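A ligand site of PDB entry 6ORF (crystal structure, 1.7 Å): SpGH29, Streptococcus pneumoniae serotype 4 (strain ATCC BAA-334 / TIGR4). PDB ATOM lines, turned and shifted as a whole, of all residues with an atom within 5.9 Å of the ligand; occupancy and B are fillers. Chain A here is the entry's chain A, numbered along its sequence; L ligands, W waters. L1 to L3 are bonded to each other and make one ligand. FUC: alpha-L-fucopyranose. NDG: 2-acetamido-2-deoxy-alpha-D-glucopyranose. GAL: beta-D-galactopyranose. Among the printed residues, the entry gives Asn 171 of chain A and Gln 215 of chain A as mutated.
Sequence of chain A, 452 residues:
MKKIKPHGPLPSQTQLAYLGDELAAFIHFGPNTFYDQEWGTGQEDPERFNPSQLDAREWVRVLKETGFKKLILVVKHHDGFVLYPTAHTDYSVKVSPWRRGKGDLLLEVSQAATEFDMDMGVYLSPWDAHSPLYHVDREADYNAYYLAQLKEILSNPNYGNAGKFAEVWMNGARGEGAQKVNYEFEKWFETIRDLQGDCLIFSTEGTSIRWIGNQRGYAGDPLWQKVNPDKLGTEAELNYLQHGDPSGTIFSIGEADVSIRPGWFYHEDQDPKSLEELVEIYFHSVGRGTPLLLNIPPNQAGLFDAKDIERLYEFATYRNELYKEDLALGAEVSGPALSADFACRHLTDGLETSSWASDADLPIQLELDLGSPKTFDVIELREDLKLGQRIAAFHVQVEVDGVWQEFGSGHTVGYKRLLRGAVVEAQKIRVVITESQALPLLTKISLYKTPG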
ATOM      1  N   PHE A  26      24.003   5.730 -20.078  1.00  0.00           N
ATOM      2  CA  PHE A  26      22.726   5.590 -19.388  1.00  0.00           C
ATOM      3  C   PHE A  26      22.187   4.195 -19.692  1.00  0.00           C
ATOM      4  O   PHE A  26      22.374   3.716 -20.802  1.00  0.00           O
ATOM      5  CB  PHE A  26      21.763   6.636 -19.963  1.00  0.00           C
ATOM      6  CG  PHE A  26      21.005   7.529 -19.009  1.00  0.00           C
ATOM      7  CD1 PHE A  26      20.726   7.156 -17.695  1.00  0.00           C
ATOM      8  CD2 PHE A  26      20.415   8.686 -19.519  1.00  0.00           C
ATOM      9  CE1 PHE A  26      19.983   7.976 -16.864  1.00  0.00           C
ATOM     10  CE2 PHE A  26      19.645   9.489 -18.692  1.00  0.00           C
ATOM     11  CZ  PHE A  26      19.426   9.132 -17.376  1.00  0.00           C
ATOM     12  N   HIS A  28      18.416   2.395 -19.437  1.00  0.00           N
ATOM     13  CA  HIS A  28      16.995   2.275 -19.160  1.00  0.00           C
ATOM     14  C   HIS A  28      16.573   0.852 -19.514  1.00  0.00           C
ATOM     15  O   HIS A  28      16.656   0.471 -20.671  1.00  0.00           O
ATOM     16  CB  HIS A  28      16.149   3.227 -20.032  1.00  0.00           C
ATOM     17  CG  HIS A  28      16.166   4.676 -19.598  1.00  0.00           C
ATOM     18  ND1 HIS A  28      17.306   5.456 -19.693  1.00  0.00           N
ATOM     19  CD2 HIS A  28      15.189   5.488 -19.142  1.00  0.00           C
ATOM     20  CE1 HIS A  28      17.040   6.695 -19.284  1.00  0.00           C
ATOM     21  NE2 HIS A  28      15.745   6.736 -18.936  1.00  0.00           N
ATOM     22  N   GLU A  38       7.334   3.534 -23.526  1.00  0.00           N
ATOM     23  CA  GLU A  38       8.323   4.481 -23.031  1.00  0.00           C
ATOM     24  C   GLU A  38       8.029   4.902 -21.589  1.00  0.00           C
ATOM     25  O   GLU A  38       8.960   5.177 -20.846  1.00  0.00           O
ATOM     26  CB  GLU A  38       8.388   5.692 -23.967  1.00  0.00           C
ATOM     27  CG  GLU A  38       9.223   5.373 -25.189  1.00  0.00           C
ATOM     28  CD  GLU A  38      10.697   5.247 -24.846  1.00  0.00           C
ATOM     29  OE1 GLU A  38      11.321   6.275 -24.490  1.00  0.00           O
ATOM     30  OE2 GLU A  38      11.241   4.101 -24.963  1.00  0.00           O
ATOM     31  N   TRP A  39       6.735   5.031 -21.242  1.00  0.00           N
ATOM     32  CA  TRP A  39       6.270   5.307 -19.894  1.00  0.00           C
ATOM     33  C   TRP A  39       5.361   4.161 -19.450  1.00  0.00           C
ATOM     34  O   TRP A  39       4.562   3.659 -20.256  1.00  0.00           O
ATOM     35  CB  TRP A  39       5.485   6.632 -19.851  1.00  0.00           C
ATOM     36  CG  TRP A  39       6.336   7.859 -19.760  1.00  0.00           C
ATOM     37  CD1 TRP A  39       7.695   7.959 -19.931  1.00  0.00           C
ATOM     38  CD2 TRP A  39       5.874   9.183 -19.431  1.00  0.00           C
ATOM     39  NE1 TRP A  39       8.109   9.250 -19.738  1.00  0.00           N
ATOM     40  CE2 TRP A  39       7.003  10.028 -19.440  1.00  0.00           C
ATOM     41  CE3 TRP A  39       4.610   9.742 -19.195  1.00  0.00           C
ATOM     42  CZ2 TRP A  39       6.909  11.382 -19.132  1.00  0.00           C
ATOM     43  CZ3 TRP A  39       4.500  11.091 -18.915  1.00  0.00           C
ATOM     44  CH2 TRP A  39       5.649  11.892 -18.909  1.00  0.00           C
ATOM     45  N   VAL A  74      19.100   3.136 -14.290  1.00  0.00           N
ATOM     46  CA  VAL A  74      17.744   3.291 -13.814  1.00  0.00           C
ATOM     47  C   VAL A  74      17.428   2.140 -12.869  1.00  0.00           C
ATOM     48  O   VAL A  74      17.473   0.986 -13.285  1.00  0.00           O
ATOM     49  CB  VAL A  74      16.756   3.342 -15.002  1.00  0.00           C
ATOM     50  CG1 VAL A  74      15.280   3.272 -14.539  1.00  0.00           C
ATOM     51  CG2 VAL A  74      17.009   4.599 -15.832  1.00  0.00           C
ATOM     52  N   HIS A  77      11.960   3.547 -12.649  1.00  0.00           N
ATOM     53  CA  HIS A  77      11.455   4.554 -13.568  1.00  0.00           C
ATOM     54  C   HIS A  77      10.136   5.102 -13.029  1.00  0.00           C
ATOM     55  O   HIS A  77       9.746   4.812 -11.884  1.00  0.00           O
ATOM     56  CB  HIS A  77      11.362   3.969 -14.995  1.00  0.00           C
ATOM     57  CG  HIS A  77      11.463   5.000 -16.077  1.00  0.00           C
ATOM     58  ND1 HIS A  77      10.347   5.467 -16.740  1.00  0.00           N
ATOM     59  CD2 HIS A  77      12.519   5.725 -16.549  1.00  0.00           C
ATOM     60  CE1 HIS A  77      10.731   6.385 -17.627  1.00  0.00           C
ATOM     61  NE2 HIS A  77      12.028   6.559 -17.527  1.00  0.00           N
ATOM     62  N   HIS A  78       9.402   5.872 -13.857  1.00  0.00           N
ATOM     63  CA  HIS A  78       8.168   6.516 -13.402  1.00  0.00           C
ATOM     64  C   HIS A  78       7.118   5.494 -12.985  1.00  0.00           C
ATOM     65  O   HIS A  78       6.310   5.795 -12.128  1.00  0.00           O
ATOM     66  CB  HIS A  78       7.540   7.390 -14.506  1.00  0.00           C
ATOM     67  CG  HIS A  78       8.481   8.345 -15.162  1.00  0.00           C
ATOM     68  ND1 HIS A  78       9.446   9.021 -14.441  1.00  0.00           N
ATOM     69  CD2 HIS A  78       8.546   8.822 -16.437  1.00  0.00           C
ATOM     70  CE1 HIS A  78      10.118   9.854 -15.237  1.00  0.00           C
ATOM     71  NE2 HIS A  78       9.596   9.742 -16.474  1.00  0.00           N
ATOM     72  N   TYR A 123      19.636   6.334 -11.056  1.00  0.00           N
ATOM     73  CA  TYR A 123      18.433   7.094 -11.406  1.00  0.00           C
ATOM     74  C   TYR A 123      17.261   6.470 -10.625  1.00  0.00           C
ATOM     75  O   TYR A 123      16.921   5.289 -10.795  1.00  0.00           O
ATOM     76  CB  TYR A 123      18.291   7.045 -12.932  1.00  0.00           C
ATOM     77  CG  TYR A 123      17.008   7.488 -13.595  1.00  0.00           C
ATOM     78  CD1 TYR A 123      15.760   7.021 -13.195  1.00  0.00           C
ATOM     79  CD2 TYR A 123      17.054   8.318 -14.707  1.00  0.00           C
ATOM     80  CE1 TYR A 123      14.586   7.406 -13.858  1.00  0.00           C
ATOM     81  CE2 TYR A 123      15.900   8.701 -15.378  1.00  0.00           C
ATOM     82  CZ  TYR A 123      14.665   8.235 -14.972  1.00  0.00           C
ATOM     83  OH  TYR A 123      13.546   8.647 -15.637  1.00  0.00           O
ATOM     84  N   TRP A 169      20.634  10.719 -10.095  1.00  0.00           N
ATOM     85  CA  TRP A 169      19.795  11.370 -11.100  1.00  0.00           C
ATOM     86  C   TRP A 169      18.357  11.495 -10.602  1.00  0.00           C
ATOM     87  O   TRP A 169      17.702  10.482 -10.340  1.00  0.00           O
ATOM     88  CB  TRP A 169      19.829  10.526 -12.376  1.00  0.00           C
ATOM     89  CG  TRP A 169      20.255  11.234 -13.627  1.00  0.00           C
ATOM     90  CD1 TRP A 169      21.519  11.578 -13.976  1.00  0.00           C
ATOM     91  CD2 TRP A 169      19.409  11.662 -14.719  1.00  0.00           C
ATOM     92  NE1 TRP A 169      21.540  12.179 -15.203  1.00  0.00           N
ATOM     93  CE2 TRP A 169      20.269  12.253 -15.677  1.00  0.00           C
ATOM     94  CE3 TRP A 169      18.035  11.593 -14.961  1.00  0.00           C
ATOM     95  CZ2 TRP A 169      19.809  12.739 -16.886  1.00  0.00           C
ATOM     96  CZ3 TRP A 169      17.573  12.112 -16.171  1.00  0.00           C
ATOM     97  CH2 TRP A 169      18.456  12.658 -17.106  1.00  0.00           C
ATOM     98  N   MET A 170      17.858  12.739 -10.510  1.00  0.00           N
ATOM     99  CA  MET A 170      16.477  12.984 -10.123  1.00  0.00           C
ATOM    100  C   MET A 170      15.754  13.640 -11.302  1.00  0.00           C
ATOM    101  O   MET A 170      15.786  14.860 -11.511  1.00  0.00           O
ATOM    102  CB  MET A 170      16.435  13.924  -8.908  1.00  0.00           C
ATOM    103  CG  MET A 170      17.216  13.333  -7.713  1.00  0.00           C
ATOM    104  SD  MET A 170      17.256  14.594  -6.415  1.00  0.00           S
ATOM    105  CE  MET A 170      18.265  13.729  -5.198  1.00  0.00           C
ATOM    106  N   ASN A 171      15.109  12.800 -12.117  1.00  0.00           N
ATOM    107  CA  ASN A 171      14.418  13.279 -13.297  1.00  0.00           C
ATOM    108  C   ASN A 171      13.281  14.235 -12.909  1.00  0.00           C
ATOM    109  O   ASN A 171      12.523  13.984 -11.969  1.00  0.00           O
ATOM    110  CB  ASN A 171      13.885  12.065 -14.050  1.00  0.00           C
ATOM    111  CG  ASN A 171      13.579  12.314 -15.496  1.00  0.00           C
ATOM    112  OD1 ASN A 171      12.802  13.209 -15.838  1.00  0.00           O
ATOM    113  ND2 ASN A 171      14.129  11.469 -16.339  1.00  0.00           N
ATOM    114  N   GLY A 172      13.113  15.282 -13.713  1.00  0.00           N
ATOM    115  CA  GLY A 172      12.067  16.270 -13.472  1.00  0.00           C
ATOM    116  C   GLY A 172      10.702  15.929 -14.082  1.00  0.00           C
ATOM    117  O   GLY A 172       9.715  16.612 -13.797  1.00  0.00           O
ATOM    118  N   ALA A 173      10.607  14.855 -14.897  1.00  0.00           N
ATOM    119  CA  ALA A 173       9.395  14.626 -15.677  1.00  0.00           C
ATOM    120  C   ALA A 173       8.218  14.207 -14.799  1.00  0.00           C
ATOM    121  O   ALA A 173       8.393  13.407 -13.882  1.00  0.00           O
ATOM    122  CB  ALA A 173       9.663  13.557 -16.724  1.00  0.00           C
ATOM    123  N   ARG A 174       7.012  14.702 -15.115  1.00  0.00           N
ATOM    124  CA  ARG A 174       5.820  14.184 -14.464  1.00  0.00           C
ATOM    125  C   ARG A 174       4.632  14.320 -15.425  1.00  0.00           C
ATOM    126  O   ARG A 174       4.459  15.375 -16.039  1.00  0.00           O
ATOM    127  CB  ARG A 174       5.582  14.933 -13.137  1.00  0.00           C
ATOM    128  CG  ARG A 174       4.306  14.504 -12.432  1.00  0.00           C
ATOM    129  CD  ARG A 174       4.373  14.837 -10.960  1.00  0.00           C
ATOM    130  NE  ARG A 174       4.172  16.289 -10.828  1.00  0.00           N
ATOM    131  CZ  ARG A 174       4.472  16.976  -9.748  1.00  0.00           C
ATOM    132  NH1 ARG A 174       4.995  16.360  -8.683  1.00  0.00           N
ATOM    133  NH2 ARG A 174       4.255  18.283  -9.712  1.00  0.00           N
ATOM    134  N   PHE A 202      22.162  15.319 -10.427  1.00  0.00           N
ATOM    135  CA  PHE A 202      21.345  15.898 -11.491  1.00  0.00           C
ATOM    136  C   PHE A 202      19.946  16.103 -10.943  1.00  0.00           C
ATOM    137  O   PHE A 202      19.346  15.167 -10.419  1.00  0.00           O
ATOM    138  CB  PHE A 202      21.229  14.903 -12.673  1.00  0.00           C
ATOM    139  CG  PHE A 202      20.329  15.346 -13.817  1.00  0.00           C
ATOM    140  CD1 PHE A 202      18.940  15.243 -13.722  1.00  0.00           C
ATOM    141  CD2 PHE A 202      20.882  15.752 -15.015  1.00  0.00           C
ATOM    142  CE1 PHE A 202      18.107  15.598 -14.782  1.00  0.00           C
ATOM    143  CE2 PHE A 202      20.051  16.091 -16.090  1.00  0.00           C
ATOM    144  CZ  PHE A 202      18.675  16.043 -15.954  1.00  0.00           C
ATOM    145  N   THR A 204      16.312  19.221 -10.973  1.00  0.00           N
ATOM    146  CA  THR A 204      15.744  20.471 -11.479  1.00  0.00           C
ATOM    147  C   THR A 204      16.190  21.662 -10.633  1.00  0.00           C
ATOM    148  O   THR A 204      15.968  22.797 -11.076  1.00  0.00           O
ATOM    149  CB  THR A 204      14.210  20.424 -11.470  1.00  0.00           C
ATOM    150  OG1 THR A 204      13.735  20.068 -10.167  1.00  0.00           O
ATOM    151  CG2 THR A 204      13.671  19.445 -12.491  1.00  0.00           C
ATOM    152  N   TRP A 211      20.142  19.639 -16.373  1.00  0.00           N
ATOM    153  CA  TRP A 211      19.844  19.214 -17.728  1.00  0.00           C
ATOM    154  C   TRP A 211      20.301  20.269 -18.728  1.00  0.00           C
ATOM    155  O   TRP A 211      20.197  21.478 -18.451  1.00  0.00           O
ATOM    156  CB  TRP A 211      18.328  19.044 -17.822  1.00  0.00           C
ATOM    157  CG  TRP A 211      17.883  18.396 -19.091  1.00  0.00           C
ATOM    158  CD1 TRP A 211      18.517  17.410 -19.781  1.00  0.00           C
ATOM    159  CD2 TRP A 211      16.645  18.641 -19.776  1.00  0.00           C
ATOM    160  NE1 TRP A 211      17.785  17.082 -20.907  1.00  0.00           N
ATOM    161  CE2 TRP A 211      16.616  17.781 -20.901  1.00  0.00           C
ATOM    162  CE3 TRP A 211      15.554  19.468 -19.515  1.00  0.00           C
ATOM    163  CZ2 TRP A 211      15.546  17.764 -21.802  1.00  0.00           C
ATOM    164  CZ3 TRP A 211      14.508  19.470 -20.420  1.00  0.00           C
ATOM    165  CH2 TRP A 211      14.502  18.621 -21.529  1.00  0.00           C
ATOM    166  N   ASN A 214      17.553  19.632 -23.676  1.00  0.00           N
ATOM    167  CA  ASN A 214      16.993  18.835 -24.764  1.00  0.00           C
ATOM    168  C   ASN A 214      17.558  17.422 -24.605  1.00  0.00           C
ATOM    169  O   ASN A 214      18.506  17.222 -23.834  1.00  0.00           O
ATOM    170  CB  ASN A 214      17.393  19.404 -26.139  1.00  0.00           C
ATOM    171  CG  ASN A 214      18.895  19.416 -26.385  1.00  0.00           C
ATOM    172  OD1 ASN A 214      19.540  18.383 -26.621  1.00  0.00           O
ATOM    173  ND2 ASN A 214      19.479  20.599 -26.283  1.00  0.00           N
ATOM    174  N   GLN A 215      16.950  16.470 -25.320  1.00  0.00           N
ATOM    175  CA  GLN A 215      17.405  15.084 -25.321  1.00  0.00           C
ATOM    176  C   GLN A 215      17.971  14.731 -26.682  1.00  0.00           C
ATOM    177  O   GLN A 215      17.846  13.572 -27.124  1.00  0.00           O
ATOM    178  CB  GLN A 215      16.292  14.133 -24.841  1.00  0.00           C
ATOM    179  CG  GLN A 215      15.031  14.150 -25.706  1.00  0.00           C
ATOM    180  CD  GLN A 215      14.117  12.950 -25.516  1.00  0.00           C
ATOM    181  OE1 GLN A 215      13.790  12.549 -24.410  1.00  0.00           O
ATOM    182  NE2 GLN A 215      13.663  12.386 -26.628  1.00  0.00           N
ATOM    183  N   LEU A 238      14.179  26.365 -21.306  1.00  0.00           N
ATOM    184  CA  LEU A 238      15.056  25.376 -21.956  1.00  0.00           C
ATOM    185  C   LEU A 238      16.353  26.047 -22.465  1.00  0.00           C
ATOM    186  O   LEU A 238      17.425  25.431 -22.436  1.00  0.00           O
ATOM    187  CB  LEU A 238      14.329  24.745 -23.149  1.00  0.00           C
ATOM    188  CG  LEU A 238      13.086  23.933 -22.793  1.00  0.00           C
ATOM    189  CD1 LEU A 238      12.383  23.430 -24.051  1.00  0.00           C
ATOM    190  CD2 LEU A 238      13.440  22.751 -21.896  1.00  0.00           C
ATOM    191  N   ASP A 257      22.116  14.537 -22.252  1.00  0.00           N
ATOM    192  CA  ASP A 257      21.671  13.158 -22.312  1.00  0.00           C
ATOM    193  C   ASP A 257      20.983  12.890 -23.637  1.00  0.00           C
ATOM    194  O   ASP A 257      20.225  13.710 -24.125  1.00  0.00           O
ATOM    195  CB  ASP A 257      20.732  12.814 -21.153  1.00  0.00           C
ATOM    196  CG  ASP A 257      19.460  13.653 -21.128  1.00  0.00           C
ATOM    197  OD1 ASP A 257      19.571  14.889 -21.352  1.00  0.00           O
ATOM    198  OD2 ASP A 257      18.365  13.083 -20.910  1.00  0.00           O
ATOM    199  N   TRP A 264      14.031   5.733 -25.126  1.00  0.00           N
ATOM    200  CA  TRP A 264      14.956   5.409 -24.049  1.00  0.00           C
ATOM    201  C   TRP A 264      14.952   3.905 -23.757  1.00  0.00           C
ATOM    202  O   TRP A 264      15.978   3.362 -23.320  1.00  0.00           O
ATOM    203  CB  TRP A 264      14.600   6.200 -22.776  1.00  0.00           C
ATOM    204  CG  TRP A 264      14.732   7.678 -22.958  1.00  0.00           C
ATOM    205  CD1 TRP A 264      13.753   8.566 -23.282  1.00  0.00           C
ATOM    206  CD2 TRP A 264      15.959   8.437 -22.927  1.00  0.00           C
ATOM    207  NE1 TRP A 264      14.271   9.837 -23.418  1.00  0.00           N
ATOM    208  CE2 TRP A 264      15.611   9.788 -23.181  1.00  0.00           C
ATOM    209  CE3 TRP A 264      17.287   8.127 -22.642  1.00  0.00           C
ATOM    210  CZ2 TRP A 264      16.562  10.808 -23.201  1.00  0.00           C
ATOM    211  CZ3 TRP A 264      18.235   9.132 -22.653  1.00  0.00           C
ATOM    212  CH2 TRP A 264      17.875  10.459 -22.942  1.00  0.00           C
ATOM    213  N   PHE A 265      13.780   3.259 -23.879  1.00  0.00           N
ATOM    214  CA  PHE A 265      13.758   1.811 -23.698  1.00  0.00           C
ATOM    215  C   PHE A 265      14.012   1.125 -25.038  1.00  0.00           C
ATOM    216  O   PHE A 265      13.895   1.750 -26.097  1.00  0.00           O
ATOM    217  CB  PHE A 265      12.473   1.385 -22.978  1.00  0.00           C
ATOM    218  CG  PHE A 265      12.452   1.838 -21.542  1.00  0.00           C
ATOM    219  CD1 PHE A 265      12.013   3.116 -21.190  1.00  0.00           C
ATOM    220  CD2 PHE A 265      12.887   1.000 -20.533  1.00  0.00           C
ATOM    221  CE1 PHE A 265      12.015   3.515 -19.864  1.00  0.00           C
ATOM    222  CE2 PHE A 265      12.853   1.385 -19.197  1.00  0.00           C
ATOM    223  CZ  PHE A 265      12.403   2.646 -18.867  1.00  0.00           C
HETATM  224  C1  FUC L   1      12.404  11.983 -19.131  1.00  0.00           C
HETATM  225  C2  FUC L   1      11.720  10.662 -18.826  1.00  0.00           C
HETATM  226  C3  FUC L   1      12.165   9.644 -19.882  1.00  0.00           C
HETATM  227  C4  FUC L   1      13.672   9.438 -19.725  1.00  0.00           C
HETATM  228  C5  FUC L   1      14.411  10.787 -19.912  1.00  0.00           C
HETATM  229  C6  FUC L   1      15.917  10.727 -19.608  1.00  0.00           C
HETATM  230  O2  FUC L   1      10.307  10.789 -18.906  1.00  0.00           O
HETATM  231  O3  FUC L   1      11.397   8.446 -19.712  1.00  0.00           O
HETATM  232  O4  FUC L   1      13.994   8.820 -18.433  1.00  0.00           O
HETATM  233  O5  FUC L   1      13.818  11.799 -19.044  1.00  0.00           O
HETATM  234  C1  NDG L   2       9.032  13.854 -22.167  1.00  0.00           C
HETATM  235  C2  NDG L   2      10.299  13.031 -21.868  1.00  0.00           C
HETATM  236  C3  NDG L   2      10.927  13.320 -20.495  1.00  0.00           C
HETATM  237  C4  NDG L   2      11.182  14.827 -20.353  1.00  0.00           C
HETATM  238  C5  NDG L   2       9.893  15.610 -20.742  1.00  0.00           C
HETATM  239  C6  NDG L   2      10.093  17.122 -20.875  1.00  0.00           C
HETATM  240  C7  NDG L   2      10.059  10.901 -23.059  1.00  0.00           C
HETATM  241  C8  NDG L   2       9.566   9.463 -23.051  1.00  0.00           C
HETATM  242  O5  NDG L   2       9.437  15.227 -22.060  1.00  0.00           O
HETATM  243  O3  NDG L   2      12.169  12.574 -20.342  1.00  0.00           O
HETATM  244  O4  NDG L   2      11.515  15.097 -18.996  1.00  0.00           O
HETATM  245  O6  NDG L   2      11.162  17.415 -21.789  1.00  0.00           O
HETATM  246  O7  NDG L   2      10.550  11.392 -24.049  1.00  0.00           O
HETATM  247  N2  NDG L   2       9.954  11.608 -21.944  1.00  0.00           N
HETATM  248  O1  NDG L   2       8.085  13.593 -21.126  1.00  0.00           O
HETATM  249  C1  GAL L   3      12.605  15.914 -18.865  1.00  0.00           C
HETATM  250  C2  GAL L   3      12.597  16.473 -17.440  1.00  0.00           C
HETATM  251  C3  GAL L   3      13.937  17.123 -17.105  1.00  0.00           C
HETATM  252  C4  GAL L   3      15.142  16.208 -17.310  1.00  0.00           C
HETATM  253  C5  GAL L   3      15.000  15.673 -18.729  1.00  0.00           C
HETATM  254  C6  GAL L   3      16.091  14.671 -19.023  1.00  0.00           C
HETATM  255  O2  GAL L   3      11.627  17.526 -17.354  1.00  0.00           O
HETATM  256  O3  GAL L   3      13.869  17.596 -15.734  1.00  0.00           O
HETATM  257  O4  GAL L   3      15.009  15.114 -16.385  1.00  0.00           O
HETATM  258  O5  GAL L   3      13.712  15.002 -18.902  1.00  0.00           O
HETATM  259  O6  GAL L   3      16.173  14.442 -20.458  1.00  0.00           O
HETATM  260  O   HOH W   1      12.463  15.740 -23.491  1.00  0.00           O
HETATM  261  O   HOH W   2      15.471  19.807 -15.718  1.00  0.00           O
HETATM  262  O   HOH W   3      10.870  14.043 -25.090  1.00  0.00           O
HETATM  263  O   HOH W   4      12.007  10.076 -25.938  1.00  0.00           O
HETATM  264  O   HOH W   5       5.720  14.751 -21.482  1.00  0.00           O
HETATM  265  O   HOH W   6       8.438  16.954 -24.040  1.00  0.00           O
HETATM  266  O   HOH W   7      11.243   6.559 -21.619  1.00  0.00           O
HETATM  267  O   HOH W   8      11.549  19.696 -15.433  1.00  0.00           O
HETATM  268  O   HOH W   9       8.751  17.483 -17.735  1.00  0.00           O
HETATM  269  O   HOH W  10      11.191  20.009 -22.923  1.00  0.00           O
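Water W7 lies within hydrogen-bond range of an oxygen (O3) of FUC L1 (2.7 Å) and the backbone carbonyl oxygen of Glu 38 (2.8 Å).
Water W4 lies within hydrogen-bond range of O7 of NDG L2 (2.7 Å), NE2 of Gln 215 (2.9 Å) and NE1 of Trp 264 (3.4 Å).
Water W3 bridges an oxygen (O7) of NDG L2 and the side-chain amide oxygen of Gln 215.
The side-chain carboxylate of Asp 257 sits at hydrogen-bond distance from an oxygen (O6) of GAL L3.
An oxygen (O2) of FUC L1 is in hydrogen-bond range of a ring nitrogen (NE2) of His 78 (2.7 Å).
The side-chain amide nitrogen (ND2) of Asn 171 is in hydrogen-bond range of an oxygen (O5) of FUC L1, at 2.7 Å.
A ring nitrogen (NE2) of His 28 sits at hydrogen-bond distance from an oxygen (O4) of FUC L1 (2.8 Å).
An oxygen (O2) of FUC L1 lies within hydrogen-bond range of the indole nitrogen (NE1) of Trp 39 (2.8 Å).
The side-chain hydroxyl (OH) of Tyr 123 is in hydrogen-bond range of an oxygen (O4) of FUC L1, at 2.8 Å.
An oxygen (O3) of FUC L1 sits at hydrogen-bond distance from a ring nitrogen (NE2) of His 77, 3.0 Å away.
The indole nitrogen of Trp 211 sits at hydrogen-bond distance from an oxygen (O6) of GAL L3 (3.1 Å).
The backbone NH (N) of Gly 172 is in hydrogen-bond range of an oxygen (O3) of GAL L3 (3.2 Å).
An oxygen (O7) of NDG L2 sits close to the side-chain amide oxygen (OE1) of Gln 215, 3.5 Å away.
OD1 of Asp 257 lies within hydrogen-bond range of NE1 of Trp 211 (2.9 Å).
The side-chain amide nitrogen of Asn 171 sits at hydrogen-bond distance from the side-chain hydroxyl of Tyr 123 (3.0 Å).
OD1 of Asn 171 is in hydrogen-bond range of N of Ala 173 (2.9 Å).
NE2 of His 77 sits at hydrogen-bond distance from OH of Tyr 123 (3.2 Å).
The indole nitrogen (NE1) of Trp 211 lies within hydrogen-bond range of the backbone carbonyl oxygen (O) of Asn 214 (3.0 Å).
The indole nitrogen of Trp 264 lies within hydrogen-bond range of the side-chain amide oxygen of Gln 215 (2.9 Å).
N of Trp 264 lies within hydrogen-bond range of OE1 of Glu 38 (2.8 Å).
The side-chain carboxylate (OE2) of Glu 38 lies within hydrogen-bond range of the backbone NH (N) of Phe 265 (2.9 Å).
Residues that only touch the ligand: Ala 173 (3.3 Å), Phe 202 (3.5 Å), Trp 264 (3.6 Å), Trp 169 (3.6 Å), Thr 204 (3.7 Å) and Glu 38 (3.9 Å).
Within 4 Å of the ligand: His 28, Glu 38, Trp 39, His 77, His 78, Tyr 123, Trp 169, Asn 171, Gly 172, Ala 173, Phe 202, Thr 204, Trp 211, Gln 215, Asp 257 and Trp 264.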
